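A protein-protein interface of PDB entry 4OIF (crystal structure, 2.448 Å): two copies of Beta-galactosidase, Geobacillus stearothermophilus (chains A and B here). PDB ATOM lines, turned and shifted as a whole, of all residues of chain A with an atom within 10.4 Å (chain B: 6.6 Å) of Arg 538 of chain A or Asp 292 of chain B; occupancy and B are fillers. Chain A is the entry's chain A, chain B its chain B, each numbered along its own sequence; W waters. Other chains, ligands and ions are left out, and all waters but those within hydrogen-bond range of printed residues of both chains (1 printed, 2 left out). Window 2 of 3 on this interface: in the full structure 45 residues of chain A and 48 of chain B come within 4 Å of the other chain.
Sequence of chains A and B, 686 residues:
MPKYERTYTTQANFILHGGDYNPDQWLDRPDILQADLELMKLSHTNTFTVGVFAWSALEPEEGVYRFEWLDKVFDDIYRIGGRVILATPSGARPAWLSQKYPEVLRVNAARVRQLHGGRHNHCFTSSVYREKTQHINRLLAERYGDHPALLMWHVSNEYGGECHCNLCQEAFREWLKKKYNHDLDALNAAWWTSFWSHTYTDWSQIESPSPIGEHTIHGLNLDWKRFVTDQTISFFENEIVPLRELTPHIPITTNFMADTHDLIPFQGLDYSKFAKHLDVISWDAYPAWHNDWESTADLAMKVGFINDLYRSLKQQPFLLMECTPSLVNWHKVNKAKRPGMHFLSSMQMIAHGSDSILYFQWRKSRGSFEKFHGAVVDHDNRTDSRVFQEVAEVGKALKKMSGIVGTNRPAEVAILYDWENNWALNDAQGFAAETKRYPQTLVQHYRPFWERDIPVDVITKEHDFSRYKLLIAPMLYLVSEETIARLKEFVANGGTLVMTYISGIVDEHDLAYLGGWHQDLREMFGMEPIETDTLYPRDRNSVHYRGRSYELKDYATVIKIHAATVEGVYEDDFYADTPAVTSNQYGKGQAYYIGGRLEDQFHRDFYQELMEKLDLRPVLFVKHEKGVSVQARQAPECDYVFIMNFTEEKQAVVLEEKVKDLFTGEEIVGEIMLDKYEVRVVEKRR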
ATOM      1  N   GLU A 434       4.021 -27.051  -6.789  1.00  0.00           N
ATOM      2  CA  GLU A 434       5.164 -27.490  -6.012  1.00  0.00           C
ATOM      3  C   GLU A 434       4.789 -28.069  -4.658  1.00  0.00           C
ATOM      4  O   GLU A 434       5.633 -28.677  -4.010  1.00  0.00           O
ATOM      5  CB  GLU A 434       6.157 -26.333  -5.845  1.00  0.00           C
ATOM      6  CG  GLU A 434       6.956 -26.065  -7.128  1.00  0.00           C
ATOM      7  CD  GLU A 434       7.871 -24.849  -7.052  1.00  0.00           C
ATOM      8  OE1 GLU A 434       8.222 -24.417  -5.932  1.00  0.00           O
ATOM      9  OE2 GLU A 434       8.243 -24.324  -8.124  1.00  0.00           O
ATOM     10  N   THR A 435       3.531 -27.925  -4.241  1.00  0.00           N
ATOM     11  CA  THR A 435       3.152 -28.382  -2.896  1.00  0.00           C
ATOM     12  C   THR A 435       2.229 -29.590  -2.855  1.00  0.00           C
ATOM     13  O   THR A 435       1.877 -30.037  -1.769  1.00  0.00           O
ATOM     14  CB  THR A 435       2.459 -27.271  -2.077  1.00  0.00           C
ATOM     15  OG1 THR A 435       1.164 -26.986  -2.632  1.00  0.00           O
ATOM     16  CG2 THR A 435       3.312 -26.014  -2.043  1.00  0.00           C
ATOM     17  N   THR A 534      -5.861 -23.123  -1.395  1.00  0.00           N
ATOM     18  CA  THR A 534      -4.457 -23.311  -1.751  1.00  0.00           C
ATOM     19  C   THR A 534      -3.629 -22.091  -1.362  1.00  0.00           C
ATOM     20  O   THR A 534      -3.938 -20.973  -1.763  1.00  0.00           O
ATOM     21  CB  THR A 534      -4.284 -23.579  -3.250  1.00  0.00           C
ATOM     22  OG1 THR A 534      -4.921 -24.817  -3.597  1.00  0.00           O
ATOM     23  CG2 THR A 534      -2.804 -23.660  -3.600  1.00  0.00           C
ATOM     24  N   LEU A 535      -2.567 -22.310  -0.594  1.00  0.00           N
ATOM     25  CA  LEU A 535      -1.825 -21.202   0.006  1.00  0.00           C
ATOM     26  C   LEU A 535      -0.471 -20.939  -0.639  1.00  0.00           C
ATOM     27  O   LEU A 535       0.141 -21.839  -1.201  1.00  0.00           O
ATOM     28  CB  LEU A 535      -1.622 -21.466   1.494  1.00  0.00           C
ATOM     29  CG  LEU A 535      -2.906 -21.803   2.256  1.00  0.00           C
ATOM     30  CD1 LEU A 535      -2.614 -21.916   3.737  1.00  0.00           C
ATOM     31  CD2 LEU A 535      -3.965 -20.738   1.991  1.00  0.00           C
ATOM     32  N   TYR A 536      -0.020 -19.689  -0.556  1.00  0.00           N
ATOM     33  CA  TYR A 536       1.320 -19.298  -0.989  1.00  0.00           C
ATOM     34  C   TYR A 536       2.334 -19.724   0.066  1.00  0.00           C
ATOM     35  O   TYR A 536       1.949 -19.967   1.206  1.00  0.00           O
ATOM     36  CB  TYR A 536       1.375 -17.784  -1.239  1.00  0.00           C
ATOM     37  CG  TYR A 536       0.766 -17.404  -2.561  1.00  0.00           C
ATOM     38  CD1 TYR A 536      -0.610 -17.229  -2.695  1.00  0.00           C
ATOM     39  CD2 TYR A 536       1.558 -17.266  -3.688  1.00  0.00           C
ATOM     40  CE1 TYR A 536      -1.172 -16.902  -3.923  1.00  0.00           C
ATOM     41  CE2 TYR A 536       1.016 -16.950  -4.910  1.00  0.00           C
ATOM     42  CZ  TYR A 536      -0.349 -16.767  -5.030  1.00  0.00           C
ATOM     43  OH  TYR A 536      -0.868 -16.443  -6.263  1.00  0.00           O
ATOM     44  N   PRO A 537       3.621 -19.843  -0.309  1.00  0.00           N
ATOM     45  CA  PRO A 537       4.648 -20.308   0.639  1.00  0.00           C
ATOM     46  C   PRO A 537       4.709 -19.554   1.970  1.00  0.00           C
ATOM     47  O   PRO A 537       4.902 -20.179   3.010  1.00  0.00           O
ATOM     48  CB  PRO A 537       5.947 -20.114  -0.147  1.00  0.00           C
ATOM     49  CG  PRO A 537       5.539 -20.377  -1.551  1.00  0.00           C
ATOM     50  CD  PRO A 537       4.155 -19.769  -1.683  1.00  0.00           C
ATOM     51  N   ARG A 538       4.542 -18.240   1.959  1.00  0.00           N
ATOM     52  CA  ARG A 538       4.623 -17.505   3.213  1.00  0.00           C
ATOM     53  C   ARG A 538       3.310 -17.564   4.006  1.00  0.00           C
ATOM     54  O   ARG A 538       3.265 -17.138   5.158  1.00  0.00           O
ATOM     55  CB  ARG A 538       5.017 -16.048   2.956  1.00  0.00           C
ATOM     56  CG  ARG A 538       6.434 -15.873   2.425  1.00  0.00           C
ATOM     57  CD  ARG A 538       6.707 -14.429   2.038  1.00  0.00           C
ATOM     58  NE  ARG A 538       8.116 -14.246   1.691  1.00  0.00           N
ATOM     59  CZ  ARG A 538       8.573 -13.982   0.468  1.00  0.00           C
ATOM     60  NH1 ARG A 538       7.730 -13.845  -0.556  1.00  0.00           N
ATOM     61  NH2 ARG A 538       9.880 -13.844   0.269  1.00  0.00           N
ATOM     62  N   ASP A 539       2.242 -18.067   3.390  1.00  0.00           N
ATOM     63  CA  ASP A 539       0.951 -18.146   4.079  1.00  0.00           C
ATOM     64  C   ASP A 539       1.017 -19.175   5.201  1.00  0.00           C
ATOM     65  O   ASP A 539       1.721 -20.179   5.091  1.00  0.00           O
ATOM     66  CB  ASP A 539      -0.178 -18.507   3.107  1.00  0.00           C
ATOM     67  CG  ASP A 539      -0.487 -17.388   2.127  1.00  0.00           C
ATOM     68  OD1 ASP A 539      -0.104 -16.234   2.416  1.00  0.00           O
ATOM     69  OD2 ASP A 539      -1.113 -17.665   1.074  1.00  0.00           O
ATOM     70  N   ARG A 540       0.293 -18.914   6.284  1.00  0.00           N
ATOM     71  CA  ARG A 540       0.240 -19.838   7.410  1.00  0.00           C
ATOM     72  C   ARG A 540      -1.149 -19.842   8.002  1.00  0.00           C
ATOM     73  O   ARG A 540      -1.854 -18.842   7.937  1.00  0.00           O
ATOM     74  CB  ARG A 540       1.243 -19.454   8.501  1.00  0.00           C
ATOM     75  CG  ARG A 540       2.692 -19.588   8.114  1.00  0.00           C
ATOM     76  CD  ARG A 540       3.122 -21.037   7.963  1.00  0.00           C
ATOM     77  NE  ARG A 540       4.562 -21.137   7.732  1.00  0.00           N
ATOM     78  CZ  ARG A 540       5.146 -21.057   6.536  1.00  0.00           C
ATOM     79  NH1 ARG A 540       4.409 -20.878   5.445  1.00  0.00           N
ATOM     80  NH2 ARG A 540       6.470 -21.162   6.427  1.00  0.00           N
ATOM     81  N   ASN A 541      -1.546 -20.965   8.580  1.00  0.00           N
ATOM     82  CA  ASN A 541      -2.729 -20.965   9.426  1.00  0.00           C
ATOM     83  C   ASN A 541      -2.392 -21.823  10.634  1.00  0.00           C
ATOM     84  O   ASN A 541      -1.218 -22.084  10.906  1.00  0.00           O
ATOM     85  CB  ASN A 541      -3.978 -21.478   8.676  1.00  0.00           C
ATOM     86  CG  ASN A 541      -5.302 -20.842   9.192  1.00  0.00           C
ATOM     87  OD1 ASN A 541      -5.576 -20.827  10.393  1.00  0.00           O
ATOM     88  ND2 ASN A 541      -6.111 -20.313   8.274  1.00  0.00           N
ATOM     89  N   GLU A 551       0.566 -25.804  13.560  1.00  0.00           N
ATOM     90  CA  GLU A 551       0.738 -24.982  12.366  1.00  0.00           C
ATOM     91  C   GLU A 551       0.211 -25.627  11.076  1.00  0.00           C
ATOM     92  O   GLU A 551       0.408 -26.816  10.831  1.00  0.00           O
ATOM     93  CB  GLU A 551       2.208 -24.617  12.176  1.00  0.00           C
ATOM     94  CG  GLU A 551       2.417 -23.498  11.150  1.00  0.00           C
ATOM     95  CD  GLU A 551       3.870 -23.322  10.758  1.00  0.00           C
ATOM     96  OE1 GLU A 551       4.358 -22.171  10.775  1.00  0.00           O
ATOM     97  OE2 GLU A 551       4.521 -24.336  10.431  1.00  0.00           O
ATOM     98  N   LEU A 552      -0.459 -24.821  10.257  1.00  0.00           N
ATOM     99  CA  LEU A 552      -0.932 -25.270   8.957  1.00  0.00           C
ATOM    100  C   LEU A 552      -0.164 -24.587   7.840  1.00  0.00           C
ATOM    101  O   LEU A 552       0.102 -23.377   7.903  1.00  0.00           O
ATOM    102  CB  LEU A 552      -2.431 -24.998   8.789  1.00  0.00           C
ATOM    103  CG  LEU A 552      -3.096 -25.418   7.474  1.00  0.00           C
ATOM    104  CD1 LEU A 552      -4.556 -25.770   7.732  1.00  0.00           C
ATOM    105  CD2 LEU A 552      -2.995 -24.354   6.380  1.00  0.00           C
ATOM    106  N   LYS A 553       0.154 -25.371   6.812  1.00  0.00           N
ATOM    107  CA  LYS A 553       0.741 -24.866   5.572  1.00  0.00           C
ATOM    108  C   LYS A 553       0.090 -25.494   4.334  1.00  0.00           C
ATOM    109  O   LYS A 553      -0.486 -26.583   4.414  1.00  0.00           O
ATOM    110  CB  LYS A 553       2.255 -25.124   5.548  1.00  0.00           C
ATOM    111  CG  LYS A 553       2.998 -24.396   6.648  1.00  0.00           C
ATOM    112  CD  LYS A 553       4.491 -24.376   6.429  1.00  0.00           C
ATOM    113  CE  LYS A 553       5.115 -25.750   6.514  1.00  0.00           C
ATOM    114  NZ  LYS A 553       6.592 -25.659   6.273  1.00  0.00           N
ATOM    115  N   ASP A 554       0.179 -24.785   3.208  1.00  0.00           N
ATOM    116  CA  ASP A 554      -0.113 -25.310   1.865  1.00  0.00           C
ATOM    117  C   ASP A 554      -1.588 -25.489   1.524  1.00  0.00           C
ATOM    118  O   ASP A 554      -2.044 -24.987   0.496  1.00  0.00           O
ATOM    119  CB  ASP A 554       0.599 -26.653   1.641  1.00  0.00           C
ATOM    120  CG  ASP A 554       2.108 -26.540   1.742  1.00  0.00           C
ATOM    121  OD1 ASP A 554       2.645 -25.420   1.585  1.00  0.00           O
ATOM    122  OD2 ASP A 554       2.761 -27.582   1.967  1.00  0.00           O
ATOM    123  N   ASP A 572      -7.514 -18.942  12.005  1.00  0.00           N
ATOM    124  CA  ASP A 572      -7.302 -17.670  11.335  1.00  0.00           C
ATOM    125  C   ASP A 572      -7.933 -17.710   9.947  1.00  0.00           C
ATOM    126  O   ASP A 572      -8.577 -18.694   9.602  1.00  0.00           O
ATOM    127  CB  ASP A 572      -5.806 -17.361  11.259  1.00  0.00           C
ATOM    128  CG  ASP A 572      -5.511 -15.875  11.345  1.00  0.00           C
ATOM    129  OD1 ASP A 572      -6.444 -15.063  11.155  1.00  0.00           O
ATOM    130  OD2 ASP A 572      -4.338 -15.520  11.598  1.00  0.00           O
ATOM    131  N   ASP A 573      -7.752 -16.639   9.172  1.00  0.00           N
ATOM    132  CA  ASP A 573      -8.347 -16.473   7.840  1.00  0.00           C
ATOM    133  C   ASP A 573      -9.880 -16.544   7.890  1.00  0.00           C
ATOM    134  O   ASP A 573     -10.469 -16.639   8.963  1.00  0.00           O
ATOM    135  CB  ASP A 573      -7.792 -17.515   6.861  1.00  0.00           C
ATOM    136  CG  ASP A 573      -7.574 -16.953   5.452  1.00  0.00           C
ATOM    137  OD1 ASP A 573      -8.388 -16.131   4.982  1.00  0.00           O
ATOM    138  OD2 ASP A 573      -6.577 -17.346   4.808  1.00  0.00           O
ATOM    139  N   ALA B 288      -3.229 -12.209  -9.679  1.00  0.00           N
ATOM    140  CA  ALA B 288      -3.024 -13.256  -8.684  1.00  0.00           C
ATOM    141  C   ALA B 288      -3.293 -12.715  -7.286  1.00  0.00           C
ATOM    142  O   ALA B 288      -2.376 -12.626  -6.467  1.00  0.00           O
ATOM    143  CB  ALA B 288      -1.616 -13.828  -8.773  1.00  0.00           C
ATOM    144  N   HIS B 290      -4.047 -12.003  -3.497  1.00  0.00           N
ATOM    145  CA  HIS B 290      -3.651 -12.600  -2.223  1.00  0.00           C
ATOM    146  C   HIS B 290      -2.318 -13.339  -2.310  1.00  0.00           C
ATOM    147  O   HIS B 290      -2.019 -14.185  -1.466  1.00  0.00           O
ATOM    148  CB  HIS B 290      -4.740 -13.541  -1.703  1.00  0.00           C
ATOM    149  CG  HIS B 290      -6.115 -12.960  -1.754  1.00  0.00           C
ATOM    150  ND1 HIS B 290      -6.424 -11.725  -1.226  1.00  0.00           N
ATOM    151  CD2 HIS B 290      -7.273 -13.448  -2.269  1.00  0.00           C
ATOM    152  CE1 HIS B 290      -7.709 -11.476  -1.411  1.00  0.00           C
ATOM    153  NE2 HIS B 290      -8.247 -12.505  -2.046  1.00  0.00           N
ATOM    154  N   ASN B 291      -1.513 -13.016  -3.322  1.00  0.00           N
ATOM    155  CA  ASN B 291      -0.170 -13.577  -3.412  1.00  0.00           C
ATOM    156  C   ASN B 291       0.693 -13.050  -2.257  1.00  0.00           C
ATOM    157  O   ASN B 291       0.300 -12.111  -1.559  1.00  0.00           O
ATOM    158  CB  ASN B 291       0.476 -13.258  -4.768  1.00  0.00           C
ATOM    159  CG  ASN B 291       0.795 -11.786  -4.939  1.00  0.00           C
ATOM    160  OD1 ASN B 291       1.701 -11.258  -4.294  1.00  0.00           O
ATOM    161  ND2 ASN B 291       0.058 -11.115  -5.812  1.00  0.00           N
ATOM    162  N   ASP B 292       1.868 -13.642  -2.073  1.00  0.00           N
ATOM    163  CA  ASP B 292       2.694 -13.338  -0.912  1.00  0.00           C
ATOM    164  C   ASP B 292       3.953 -12.545  -1.243  1.00  0.00           C
ATOM    165  O   ASP B 292       4.894 -12.534  -0.453  1.00  0.00           O
ATOM    166  CB  ASP B 292       3.077 -14.641  -0.175  1.00  0.00           C
ATOM    167  CG  ASP B 292       4.028 -15.541  -0.976  1.00  0.00           C
ATOM    168  OD1 ASP B 292       4.176 -15.353  -2.203  1.00  0.00           O
ATOM    169  OD2 ASP B 292       4.630 -16.456  -0.366  1.00  0.00           O
ATOM    170  N   TRP B 293       3.979 -11.878  -2.392  1.00  0.00           N
ATOM    171  CA  TRP B 293       5.149 -11.075  -2.743  1.00  0.00           C
ATOM    172  C   TRP B 293       4.859  -9.562  -2.839  1.00  0.00           C
ATOM    173  O   TRP B 293       5.771  -8.760  -3.031  1.00  0.00           O
ATOM    174  CB  TRP B 293       5.760 -11.580  -4.054  1.00  0.00           C
ATOM    175  CG  TRP B 293       4.805 -11.571  -5.225  1.00  0.00           C
ATOM    176  CD1 TRP B 293       4.370 -10.476  -5.918  1.00  0.00           C
ATOM    177  CD2 TRP B 293       4.177 -12.708  -5.841  1.00  0.00           C
ATOM    178  NE1 TRP B 293       3.513 -10.861  -6.921  1.00  0.00           N
ATOM    179  CE2 TRP B 293       3.374 -12.223  -6.894  1.00  0.00           C
ATOM    180  CE3 TRP B 293       4.210 -14.087  -5.600  1.00  0.00           C
ATOM    181  CZ2 TRP B 293       2.616 -13.065  -7.704  1.00  0.00           C
ATOM    182  CZ3 TRP B 293       3.453 -14.924  -6.408  1.00  0.00           C
ATOM    183  CH2 TRP B 293       2.670 -14.410  -7.446  1.00  0.00           C
ATOM    184  N   GLU B 294       3.600  -9.175  -2.687  1.00  0.00           N
ATOM    185  CA  GLU B 294       3.211  -7.764  -2.751  1.00  0.00           C
ATOM    186  C   GLU B 294       1.881  -7.540  -2.033  1.00  0.00           C
ATOM    187  O   GLU B 294       1.106  -8.477  -1.841  1.00  0.00           O
ATOM    188  CB  GLU B 294       3.097  -7.297  -4.211  1.00  0.00           C
ATOM    189  CG  GLU B 294       1.887  -7.861  -4.919  1.00  0.00           C
ATOM    190  CD  GLU B 294       1.920  -7.663  -6.421  1.00  0.00           C
ATOM    191  OE1 GLU B 294       2.739  -6.859  -6.917  1.00  0.00           O
ATOM    192  OE2 GLU B 294       1.117  -8.318  -7.108  1.00  0.00           O
ATOM    193  N   LYS B 335      -4.863 -19.840  -5.697  1.00  0.00           N
ATOM    194  CA  LYS B 335      -5.521 -19.353  -4.499  1.00  0.00           C
ATOM    195  C   LYS B 335      -6.763 -18.577  -4.878  1.00  0.00           C
ATOM    196  O   LYS B 335      -6.743 -17.817  -5.839  1.00  0.00           O
ATOM    197  CB  LYS B 335      -4.556 -18.464  -3.702  1.00  0.00           C
ATOM    198  CG  LYS B 335      -5.087 -18.001  -2.363  1.00  0.00           C
ATOM    199  CD  LYS B 335      -3.946 -17.443  -1.563  1.00  0.00           C
ATOM    200  CE  LYS B 335      -4.390 -16.861  -0.244  1.00  0.00           C
ATOM    201  NZ  LYS B 335      -3.254 -16.107   0.337  1.00  0.00           N
HETATM  202  O   HOH W   1      -3.416 -15.807  -6.164  1.00  0.00           O
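Lys 335 of chain B touches Thr 534 of chain A (CB to O, 3.2 Å). OH of Tyr 536 of chain A touches CB of Ala 288 of chain B, at 3.7 Å. His 290 of chain B touches Tyr 536 of chain A. Tyr 536 of chain A touches Asn 291 of chain B (CE1 to CA, 3.5 Å). Asp 292 of chain B touches Tyr 536 of chain A. Tyr 536 of chain A touches Trp 293 of chain B. CD of Lys 335 of chain B touches CD1 of Tyr 536 of chain A, at 3.5 Å. OD2 of Asp 292 of chain B touches N of Pro 537 of chain A, at 3.5 Å.
Water W1 lies within hydrogen-bond range of OH of Tyr 536 of chain A (2.6 Å) and O of Ala 288 of chain B (3.4 Å).
No position is printed for both chains. Of the 10 pairs that touch across the chains among the printed residues, none has its exchanged pair printed and touching as well.
The backbone NH (N) of Tyr 536 of chain A sits at hydrogen-bond distance from the side-chain carboxylate (OD2) of Asp 539 of chain A. ND2 of Asn 291 of chain B lies within hydrogen-bond range of O of Ala 288 of chain B, 2.9 Å away. The backbone carbonyl oxygen (O) of His 290 of chain B lies within hydrogen-bond range of the side-chain amino group (NZ) of Lys 335 of chain B (2.9 Å). OD1 of Asn 291 of chain B sits at hydrogen-bond distance from N of Trp 293 of chain B (3.0 Å). The side-chain amide oxygen (OD1) of Asn 291 of chain B lies within hydrogen-bond range of the backbone NH (N) of Glu 294 of chain B (3.2 Å). The indole nitrogen (NE1) of Trp 293 of chain B sits at hydrogen-bond distance from the side-chain carboxylate (OE2) of Glu 294 of chain B (3.5 Å).
Of the printed residues of chain B, Pro 537 of chain A touches Asp 292. Of chain B, only Asp 292 (2.9 Å) comes within 4 Å of Arg 538 of chain A. Asn 291 of chain B touches one residue of chain A. Of chain A, only Tyr 536, Pro 537 and Arg 538 come within 4 Å of Asp 292 of chain B. Of chain A, only Tyr 536 (3.5 Å) comes within 4 Å of Trp 293 of chain B. Of the printed residues of chain A, Lys 335 of chain B touches Thr 534 (3.2 Å), Tyr 536 (3.5 Å) and Asp 539 (2.7 Å). The nearest residue of chain B that does not touch Arg 538 of chain A is Trp 293 of chain B (4.4 Å).
The backbone NH of Arg 538 of chain A is in hydrogen-bond range of the side-chain carboxylate of Asp 292 of chain B (2.9 Å). OD2 of Asp 539 of chain A lies within salt-bridge range of NZ of Lys 335 of chain B, at 2.7 Å.
Of the 16 printed residues of chain A, 5 touch a printed residue of chain B. Of the 7 printed residues of chain B, 6 touch a printed residue of chain A. Hydrophobic or aromatic side chains of chain B within 4 Å of the printed part of chain A: Ala 288 and Trp 293. Among the printed residues, 10 pairs touch across the chains. Among the printed residues, Asp or Glu carboxylates within 4 Å of a Lys or Arg side-chain nitrogen of the other chain: Asp 539 of chain A with Lys 335 of chain B.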
